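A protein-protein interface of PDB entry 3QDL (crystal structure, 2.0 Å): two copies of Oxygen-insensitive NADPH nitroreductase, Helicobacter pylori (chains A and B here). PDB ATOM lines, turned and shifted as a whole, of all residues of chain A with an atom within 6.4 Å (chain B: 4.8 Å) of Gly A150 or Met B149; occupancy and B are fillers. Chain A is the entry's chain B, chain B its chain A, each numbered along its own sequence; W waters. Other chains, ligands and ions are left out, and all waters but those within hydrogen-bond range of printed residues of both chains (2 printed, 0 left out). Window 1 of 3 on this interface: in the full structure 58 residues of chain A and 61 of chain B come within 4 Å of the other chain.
Water W1 bridges OE1 of Gln A146 (2.6 Å) and O of Gly B145 (3.4 Å).
Water W2 lies within hydrogen-bond range of O of Gly A145 (2.7 Å) and OE1 of Gln B146 (2.9 Å).
O of Ile A39 sits at hydrogen-bond distance from NE2 of Gln A146 (3.1 Å).
Gly B145 touches its own counterpart, Gly A145.
Gln A146 touches Met B149, and with the chains exchanged Met A149 touches Gln B146.
Met A149 touches its own counterpart, Met B149.
Leu A153 touches its own counterpart, Leu B153.
Positions printed for both chains: 145, 146, 147, 148, 149, 150, 151, 152 and 153.
Of the 13 pairs that touch across the chains among the printed residues, 9 have their exchanged pair printed and touching as well.
C of Gly A145 touches C of Gly B145, at 3.7 Å.
Gln B146 touches Gly A145.
Arg B16 touches Gln A146.
Met B149 touches Gln A146 (CG to CA, 3.9 Å).
Met A149 touches Met B149.
Met A149 touches Gly B150.
N of Gly A150 touches CE of Met B149 (3.9 Å).
Leu A153 touches Leu B12.
Leu A153 touches Met B149 (CD1 to CE, 3.8 Å).
Leu B153 touches Leu A153 (CD2 to CD2, 3.8 Å).
The side-chain amide oxygen of Gln B146 lies close to the side-chain sulfur of Met A149 (3.7 Å).
Of the 13 printed residues of chain A, 6 touch a printed residue of chain B.
Among the printed residues, no Asp or Glu carboxylate lies within 4 Å of a Lys or Arg side-chain nitrogen of the other chain.
Of chain B, only Met B149 comes within 4 Å of Gly A150.
Met B149 touches four residues of chain A.
Of the printed residues of chain A, Leu B12 touches Leu A153.
Printed residues of chain A within 4 Å of Arg B16: Gln A146 (3.6 Å).
Printed residues of chain A within 4 Å of Leu B153: Leu A153 (3.8 Å).
Printed residues of chain A within 4 Å of Gly B150: Met A149 (3.99 Å).
Ile B147 touches none of the printed residues of chain A.
Cys B148 touches none of the printed residues of chain A.
The nearest printed residue of chain B that does not touch Gly A150 is Leu B13 (5.7 Å).
The nearest residue of chain A that does not touch Met B149 is Gly A145 (5.0 Å).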
ATOM      1  N   GLU A  35      -1.034 -28.550 -17.827  1.00  0.00           N
ATOM      2  CA  GLU A  35      -1.987 -28.638 -16.720  1.00  0.00           C
ATOM      3  C   GLU A  35      -1.549 -27.747 -15.559  1.00  0.00           C
ATOM      4  O   GLU A  35      -2.352 -26.971 -15.036  1.00  0.00           O
ATOM      5  CB  GLU A  35      -2.177 -30.078 -16.245  1.00  0.00           C
ATOM      6  CG  GLU A  35      -3.170 -30.195 -15.087  1.00  0.00           C
ATOM      7  CD  GLU A  35      -3.756 -31.581 -14.930  1.00  0.00           C
ATOM      8  OE1 GLU A  35      -4.660 -31.744 -14.081  1.00  0.00           O
ATOM      9  OE2 GLU A  35      -3.314 -32.504 -15.644  1.00  0.00           O
ATOM     10  N   ILE A  39      -3.833 -24.893 -13.810  1.00  0.00           N
ATOM     11  CA  ILE A  39      -4.142 -24.882 -12.373  1.00  0.00           C
ATOM     12  C   ILE A  39      -3.845 -23.502 -11.777  1.00  0.00           C
ATOM     13  O   ILE A  39      -4.633 -22.966 -10.988  1.00  0.00           O
ATOM     14  CB  ILE A  39      -3.349 -25.968 -11.606  1.00  0.00           C
ATOM     15  CG1 ILE A  39      -3.826 -27.369 -11.997  1.00  0.00           C
ATOM     16  CG2 ILE A  39      -3.479 -25.774 -10.093  1.00  0.00           C
ATOM     17  CD1 ILE A  39      -2.849 -28.471 -11.638  1.00  0.00           C
ATOM     18  N   GLY A 145      -0.979 -22.099  -3.089  1.00  0.00           N
ATOM     19  CA  GLY A 145      -1.683 -23.157  -2.354  1.00  0.00           C
ATOM     20  C   GLY A 145      -2.560 -24.048  -3.224  1.00  0.00           C
ATOM     21  O   GLY A 145      -2.621 -25.261  -3.014  1.00  0.00           O
ATOM     22  N   GLN A 146      -3.248 -23.443  -4.190  1.00  0.00           N
ATOM     23  CA  GLN A 146      -4.044 -24.190  -5.173  1.00  0.00           C
ATOM     24  C   GLN A 146      -3.156 -25.051  -6.072  1.00  0.00           C
ATOM     25  O   GLN A 146      -3.472 -26.217  -6.327  1.00  0.00           O
ATOM     26  CB  GLN A 146      -4.920 -23.239  -6.005  1.00  0.00           C
ATOM     27  CG  GLN A 146      -5.545 -23.872  -7.257  1.00  0.00           C
ATOM     28  CD  GLN A 146      -6.839 -23.204  -7.684  1.00  0.00           C
ATOM     29  OE1 GLN A 146      -7.642 -22.778  -6.852  1.00  0.00           O
ATOM     30  NE2 GLN A 146      -7.059 -23.135  -8.993  1.00  0.00           N
ATOM     31  N   ILE A 147      -2.042 -24.472  -6.528  1.00  0.00           N
ATOM     32  CA  ILE A 147      -1.088 -25.155  -7.409  1.00  0.00           C
ATOM     33  C   ILE A 147      -0.541 -26.439  -6.784  1.00  0.00           C
ATOM     34  O   ILE A 147      -0.655 -27.516  -7.379  1.00  0.00           O
ATOM     35  CB  ILE A 147       0.082 -24.217  -7.836  1.00  0.00           C
ATOM     36  CG1 ILE A 147      -0.426 -23.122  -8.778  1.00  0.00           C
ATOM     37  CG2 ILE A 147       1.213 -25.014  -8.512  1.00  0.00           C
ATOM     38  CD1 ILE A 147       0.409 -21.850  -8.767  1.00  0.00           C
ATOM     39  N   CYS A 148       0.032 -26.326  -5.586  1.00  0.00           N
ATOM     40  CA  CYS A 148       0.647 -27.478  -4.916  1.00  0.00           C
ATOM     41  C   CYS A 148      -0.346 -28.619  -4.670  1.00  0.00           C
ATOM     42  O   CYS A 148       0.014 -29.794  -4.784  1.00  0.00           O
ATOM     43  CB  CYS A 148       1.349 -27.055  -3.623  1.00  0.00           C
ATOM     44  SG  CYS A 148       2.918 -26.173  -3.885  1.00  0.00           S
ATOM     45  N   MET A 149      -1.593 -28.265  -4.356  1.00  0.00           N
ATOM     46  CA  MET A 149      -2.680 -29.244  -4.236  1.00  0.00           C
ATOM     47  C   MET A 149      -2.965 -29.923  -5.575  1.00  0.00           C
ATOM     48  O   MET A 149      -3.122 -31.145  -5.634  1.00  0.00           O
ATOM     49  CB  MET A 149      -3.953 -28.595  -3.681  1.00  0.00           C
ATOM     50  CG  MET A 149      -3.919 -28.328  -2.174  1.00  0.00           C
ATOM     51  SD  MET A 149      -3.977 -29.824  -1.162  1.00  0.00           S
ATOM     52  CE  MET A 149      -5.735 -30.162  -1.177  1.00  0.00           C
ATOM     53  N   GLY A 150      -3.012 -29.127  -6.642  1.00  0.00           N
ATOM     54  CA  GLY A 150      -3.233 -29.649  -7.993  1.00  0.00           C
ATOM     55  C   GLY A 150      -2.092 -30.525  -8.477  1.00  0.00           C
ATOM     56  O   GLY A 150      -2.318 -31.534  -9.151  1.00  0.00           O
ATOM     57  N   VAL A 151      -0.868 -30.129  -8.131  1.00  0.00           N
ATOM     58  CA  VAL A 151       0.340 -30.895  -8.452  1.00  0.00           C
ATOM     59  C   VAL A 151       0.299 -32.287  -7.812  1.00  0.00           C
ATOM     60  O   VAL A 151       0.571 -33.294  -8.475  1.00  0.00           O
ATOM     61  CB  VAL A 151       1.622 -30.129  -8.028  1.00  0.00           C
ATOM     62  CG1 VAL A 151       2.854 -31.044  -8.042  1.00  0.00           C
ATOM     63  CG2 VAL A 151       1.843 -28.925  -8.941  1.00  0.00           C
ATOM     64  N   SER A 152      -0.064 -32.335  -6.532  1.00  0.00           N
ATOM     65  CA  SER A 152      -0.181 -33.596  -5.795  1.00  0.00           C
ATOM     66  C   SER A 152      -1.336 -34.481  -6.281  1.00  0.00           C
ATOM     67  O   SER A 152      -1.284 -35.709  -6.139  1.00  0.00           O
ATOM     68  CB  SER A 152      -0.302 -33.333  -4.290  1.00  0.00           C
ATOM     69  OG  SER A 152       0.949 -32.975  -3.728  1.00  0.00           O
ATOM     70  N   LEU A 153      -2.373 -33.863  -6.848  1.00  0.00           N
ATOM     71  CA  LEU A 153      -3.486 -34.614  -7.439  1.00  0.00           C
ATOM     72  C   LEU A 153      -3.055 -35.379  -8.693  1.00  0.00           C
ATOM     73  O   LEU A 153      -3.604 -36.442  -8.999  1.00  0.00           O
ATOM     74  CB  LEU A 153      -4.666 -33.692  -7.763  1.00  0.00           C
ATOM     75  CG  LEU A 153      -5.567 -33.232  -6.612  1.00  0.00           C
ATOM     76  CD1 LEU A 153      -6.438 -32.087  -7.075  1.00  0.00           C
ATOM     77  CD2 LEU A 153      -6.423 -34.371  -6.072  1.00  0.00           C
ATOM     78  N   MET A 154      -2.072 -34.822  -9.402  1.00  0.00           N
ATOM     79  CA  MET A 154      -1.460 -35.446 -10.579  1.00  0.00           C
ATOM     80  C   MET A 154      -0.528 -36.592 -10.189  1.00  0.00           C
ATOM     81  O   MET A 154      -0.116 -37.381 -11.042  1.00  0.00           O
ATOM     82  CB  MET A 154      -0.655 -34.409 -11.374  1.00  0.00           C
ATOM     83  CG  MET A 154      -1.465 -33.271 -11.987  1.00  0.00           C
ATOM     84  SD  MET A 154      -0.411 -31.963 -12.666  1.00  0.00           S
ATOM     85  CE  MET A 154       0.084 -32.669 -14.243  1.00  0.00           C
ATOM     86  N   GLY A 155      -0.186 -36.671  -8.906  1.00  0.00           N
ATOM     87  CA  GLY A 155       0.762 -37.668  -8.415  1.00  0.00           C
ATOM     88  C   GLY A 155       2.202 -37.259  -8.660  1.00  0.00           C
ATOM     89  O   GLY A 155       3.059 -38.103  -8.930  1.00  0.00           O
ATOM     90  N   LEU B  12     -12.395 -30.780 -11.315  1.00  0.00           N
ATOM     91  CA  LEU B  12     -12.182 -30.204  -9.986  1.00  0.00           C
ATOM     92  C   LEU B  12     -11.839 -28.718 -10.042  1.00  0.00           C
ATOM     93  O   LEU B  12     -12.363 -27.930  -9.254  1.00  0.00           O
ATOM     94  CB  LEU B  12     -11.111 -30.967  -9.207  1.00  0.00           C
ATOM     95  CG  LEU B  12     -11.018 -30.574  -7.728  1.00  0.00           C
ATOM     96  CD1 LEU B  12     -12.177 -31.158  -6.934  1.00  0.00           C
ATOM     97  CD2 LEU B  12      -9.706 -31.029  -7.149  1.00  0.00           C
ATOM     98  N   LEU B  13     -10.966 -28.342 -10.978  1.00  0.00           N
ATOM     99  CA  LEU B  13     -10.611 -26.937 -11.190  1.00  0.00           C
ATOM    100  C   LEU B  13     -11.831 -26.060 -11.483  1.00  0.00           C
ATOM    101  O   LEU B  13     -11.846 -24.879 -11.134  1.00  0.00           O
ATOM    102  CB  LEU B  13      -9.568 -26.804 -12.307  1.00  0.00           C
ATOM    103  CG  LEU B  13      -8.115 -26.454 -11.960  1.00  0.00           C
ATOM    104  CD1 LEU B  13      -7.530 -27.303 -10.831  1.00  0.00           C
ATOM    105  CD2 LEU B  13      -7.251 -26.552 -13.218  1.00  0.00           C
ATOM    106  N   ARG B  16     -14.169 -26.114  -8.146  1.00  0.00           N
ATOM    107  CA  ARG B  16     -13.608 -25.082  -7.280  1.00  0.00           C
ATOM    108  C   ARG B  16     -14.031 -23.741  -7.866  1.00  0.00           C
ATOM    109  O   ARG B  16     -13.420 -23.248  -8.818  1.00  0.00           O
ATOM    110  CB  ARG B  16     -12.077 -25.197  -7.218  1.00  0.00           C
ATOM    111  CG  ARG B  16     -11.408 -24.626  -5.951  1.00  0.00           C
ATOM    112  CD  ARG B  16     -11.644 -23.128  -5.749  1.00  0.00           C
ATOM    113  NE  ARG B  16     -11.250 -22.336  -6.915  1.00  0.00           N
ATOM    114  CZ  ARG B  16     -11.790 -21.170  -7.251  1.00  0.00           C
ATOM    115  NH1 ARG B  16     -11.365 -20.531  -8.336  1.00  0.00           N
ATOM    116  NH2 ARG B  16     -12.765 -20.645  -6.518  1.00  0.00           N
ATOM    117  N   GLY B 145      -5.737 -21.020  -0.394  1.00  0.00           N
ATOM    118  CA  GLY B 145      -5.658 -21.744  -1.666  1.00  0.00           C
ATOM    119  C   GLY B 145      -5.740 -23.255  -1.517  1.00  0.00           C
ATOM    120  O   GLY B 145      -6.366 -23.932  -2.336  1.00  0.00           O
ATOM    121  N   GLN B 146      -5.107 -23.782  -0.471  1.00  0.00           N
ATOM    122  CA  GLN B 146      -5.182 -25.212  -0.163  1.00  0.00           C
ATOM    123  C   GLN B 146      -6.582 -25.615   0.312  1.00  0.00           C
ATOM    124  O   GLN B 146      -7.152 -26.594  -0.185  1.00  0.00           O
ATOM    125  CB  GLN B 146      -4.104 -25.619   0.855  1.00  0.00           C
ATOM    126  CG  GLN B 146      -4.295 -27.026   1.446  1.00  0.00           C
ATOM    127  CD  GLN B 146      -2.993 -27.737   1.779  1.00  0.00           C
ATOM    128  OE1 GLN B 146      -2.009 -27.646   1.041  1.00  0.00           O
ATOM    129  NE2 GLN B 146      -2.990 -28.473   2.889  1.00  0.00           N
ATOM    130  N   ILE B 147      -7.124 -24.850   1.259  1.00  0.00           N
ATOM    131  CA  ILE B 147      -8.451 -25.094   1.837  1.00  0.00           C
ATOM    132  C   ILE B 147      -9.542 -25.228   0.777  1.00  0.00           C
ATOM    133  O   ILE B 147     -10.330 -26.177   0.810  1.00  0.00           O
ATOM    134  CB  ILE B 147      -8.849 -23.986   2.854  1.00  0.00           C
ATOM    135  CG1 ILE B 147      -8.016 -24.102   4.131  1.00  0.00           C
ATOM    136  CG2 ILE B 147     -10.342 -24.055   3.196  1.00  0.00           C
ATOM    137  CD1 ILE B 147      -7.886 -22.795   4.912  1.00  0.00           C
ATOM    138  N   CYS B 148      -9.582 -24.281  -0.160  1.00  0.00           N
ATOM    139  CA  CYS B 148     -10.630 -24.255  -1.179  1.00  0.00           C
ATOM    140  C   CYS B 148     -10.523 -25.400  -2.190  1.00  0.00           C
ATOM    141  O   CYS B 148     -11.526 -25.809  -2.780  1.00  0.00           O
ATOM    142  CB  CYS B 148     -10.673 -22.896  -1.875  1.00  0.00           C
ATOM    143  SG  CYS B 148     -11.233 -21.551  -0.801  1.00  0.00           S
ATOM    144  N   MET B 149      -9.312 -25.919  -2.372  1.00  0.00           N
ATOM    145  CA  MET B 149      -9.096 -27.146  -3.141  1.00  0.00           C
ATOM    146  C   MET B 149      -9.563 -28.381  -2.360  1.00  0.00           C
ATOM    147  O   MET B 149     -10.148 -29.302  -2.930  1.00  0.00           O
ATOM    148  CB  MET B 149      -7.621 -27.288  -3.540  1.00  0.00           C
ATOM    149  CG  MET B 149      -7.193 -26.384  -4.702  1.00  0.00           C
ATOM    150  SD  MET B 149      -7.868 -26.871  -6.310  1.00  0.00           S
ATOM    151  CE  MET B 149      -6.875 -28.312  -6.675  1.00  0.00           C
ATOM    152  N   GLY B 150      -9.304 -28.391  -1.055  1.00  0.00           N
ATOM    153  CA  GLY B 150      -9.734 -29.484  -0.184  1.00  0.00           C
ATOM    154  C   GLY B 150     -11.247 -29.578  -0.106  1.00  0.00           C
ATOM    155  O   GLY B 150     -11.814 -30.671  -0.172  1.00  0.00           O
ATOM    156  N   VAL B 151     -11.893 -28.419   0.011  1.00  0.00           N
ATOM    157  CA  VAL B 151     -13.353 -28.315   0.101  1.00  0.00           C
ATOM    158  C   VAL B 151     -14.046 -28.868  -1.152  1.00  0.00           C
ATOM    159  O   VAL B 151     -15.148 -29.426  -1.074  1.00  0.00           O
ATOM    160  CB  VAL B 151     -13.792 -26.850   0.390  1.00  0.00           C
ATOM    161  CG1 VAL B 151     -15.293 -26.662   0.190  1.00  0.00           C
ATOM    162  CG2 VAL B 151     -13.400 -26.446   1.812  1.00  0.00           C
ATOM    163  N   SER B 152     -13.389 -28.725  -2.300  1.00  0.00           N
ATOM    164  CA  SER B 152     -13.920 -29.257  -3.552  1.00  0.00           C
ATOM    165  C   SER B 152     -13.746 -30.767  -3.642  1.00  0.00           C
ATOM    166  O   SER B 152     -14.582 -31.454  -4.229  1.00  0.00           O
ATOM    167  CB  SER B 152     -13.278 -28.566  -4.758  1.00  0.00           C
ATOM    168  OG  SER B 152     -13.664 -27.207  -4.809  1.00  0.00           O
ATOM    169  N   LEU B 153     -12.666 -31.278  -3.053  1.00  0.00           N
ATOM    170  CA  LEU B 153     -12.398 -32.717  -3.035  1.00  0.00           C
ATOM    171  C   LEU B 153     -13.418 -33.508  -2.215  1.00  0.00           C
ATOM    172  O   LEU B 153     -13.754 -34.645  -2.564  1.00  0.00           O
ATOM    173  CB  LEU B 153     -10.982 -33.000  -2.525  1.00  0.00           C
ATOM    174  CG  LEU B 153      -9.847 -32.770  -3.526  1.00  0.00           C
ATOM    175  CD1 LEU B 153      -8.520 -32.782  -2.818  1.00  0.00           C
ATOM    176  CD2 LEU B 153      -9.869 -33.811  -4.642  1.00  0.00           C
HETATM  177  O   HOH W   1      -8.551 -22.483  -4.460  1.00  0.00           O
HETATM  178  O   HOH W   2      -0.903 -26.219  -1.175  1.00  0.00           O
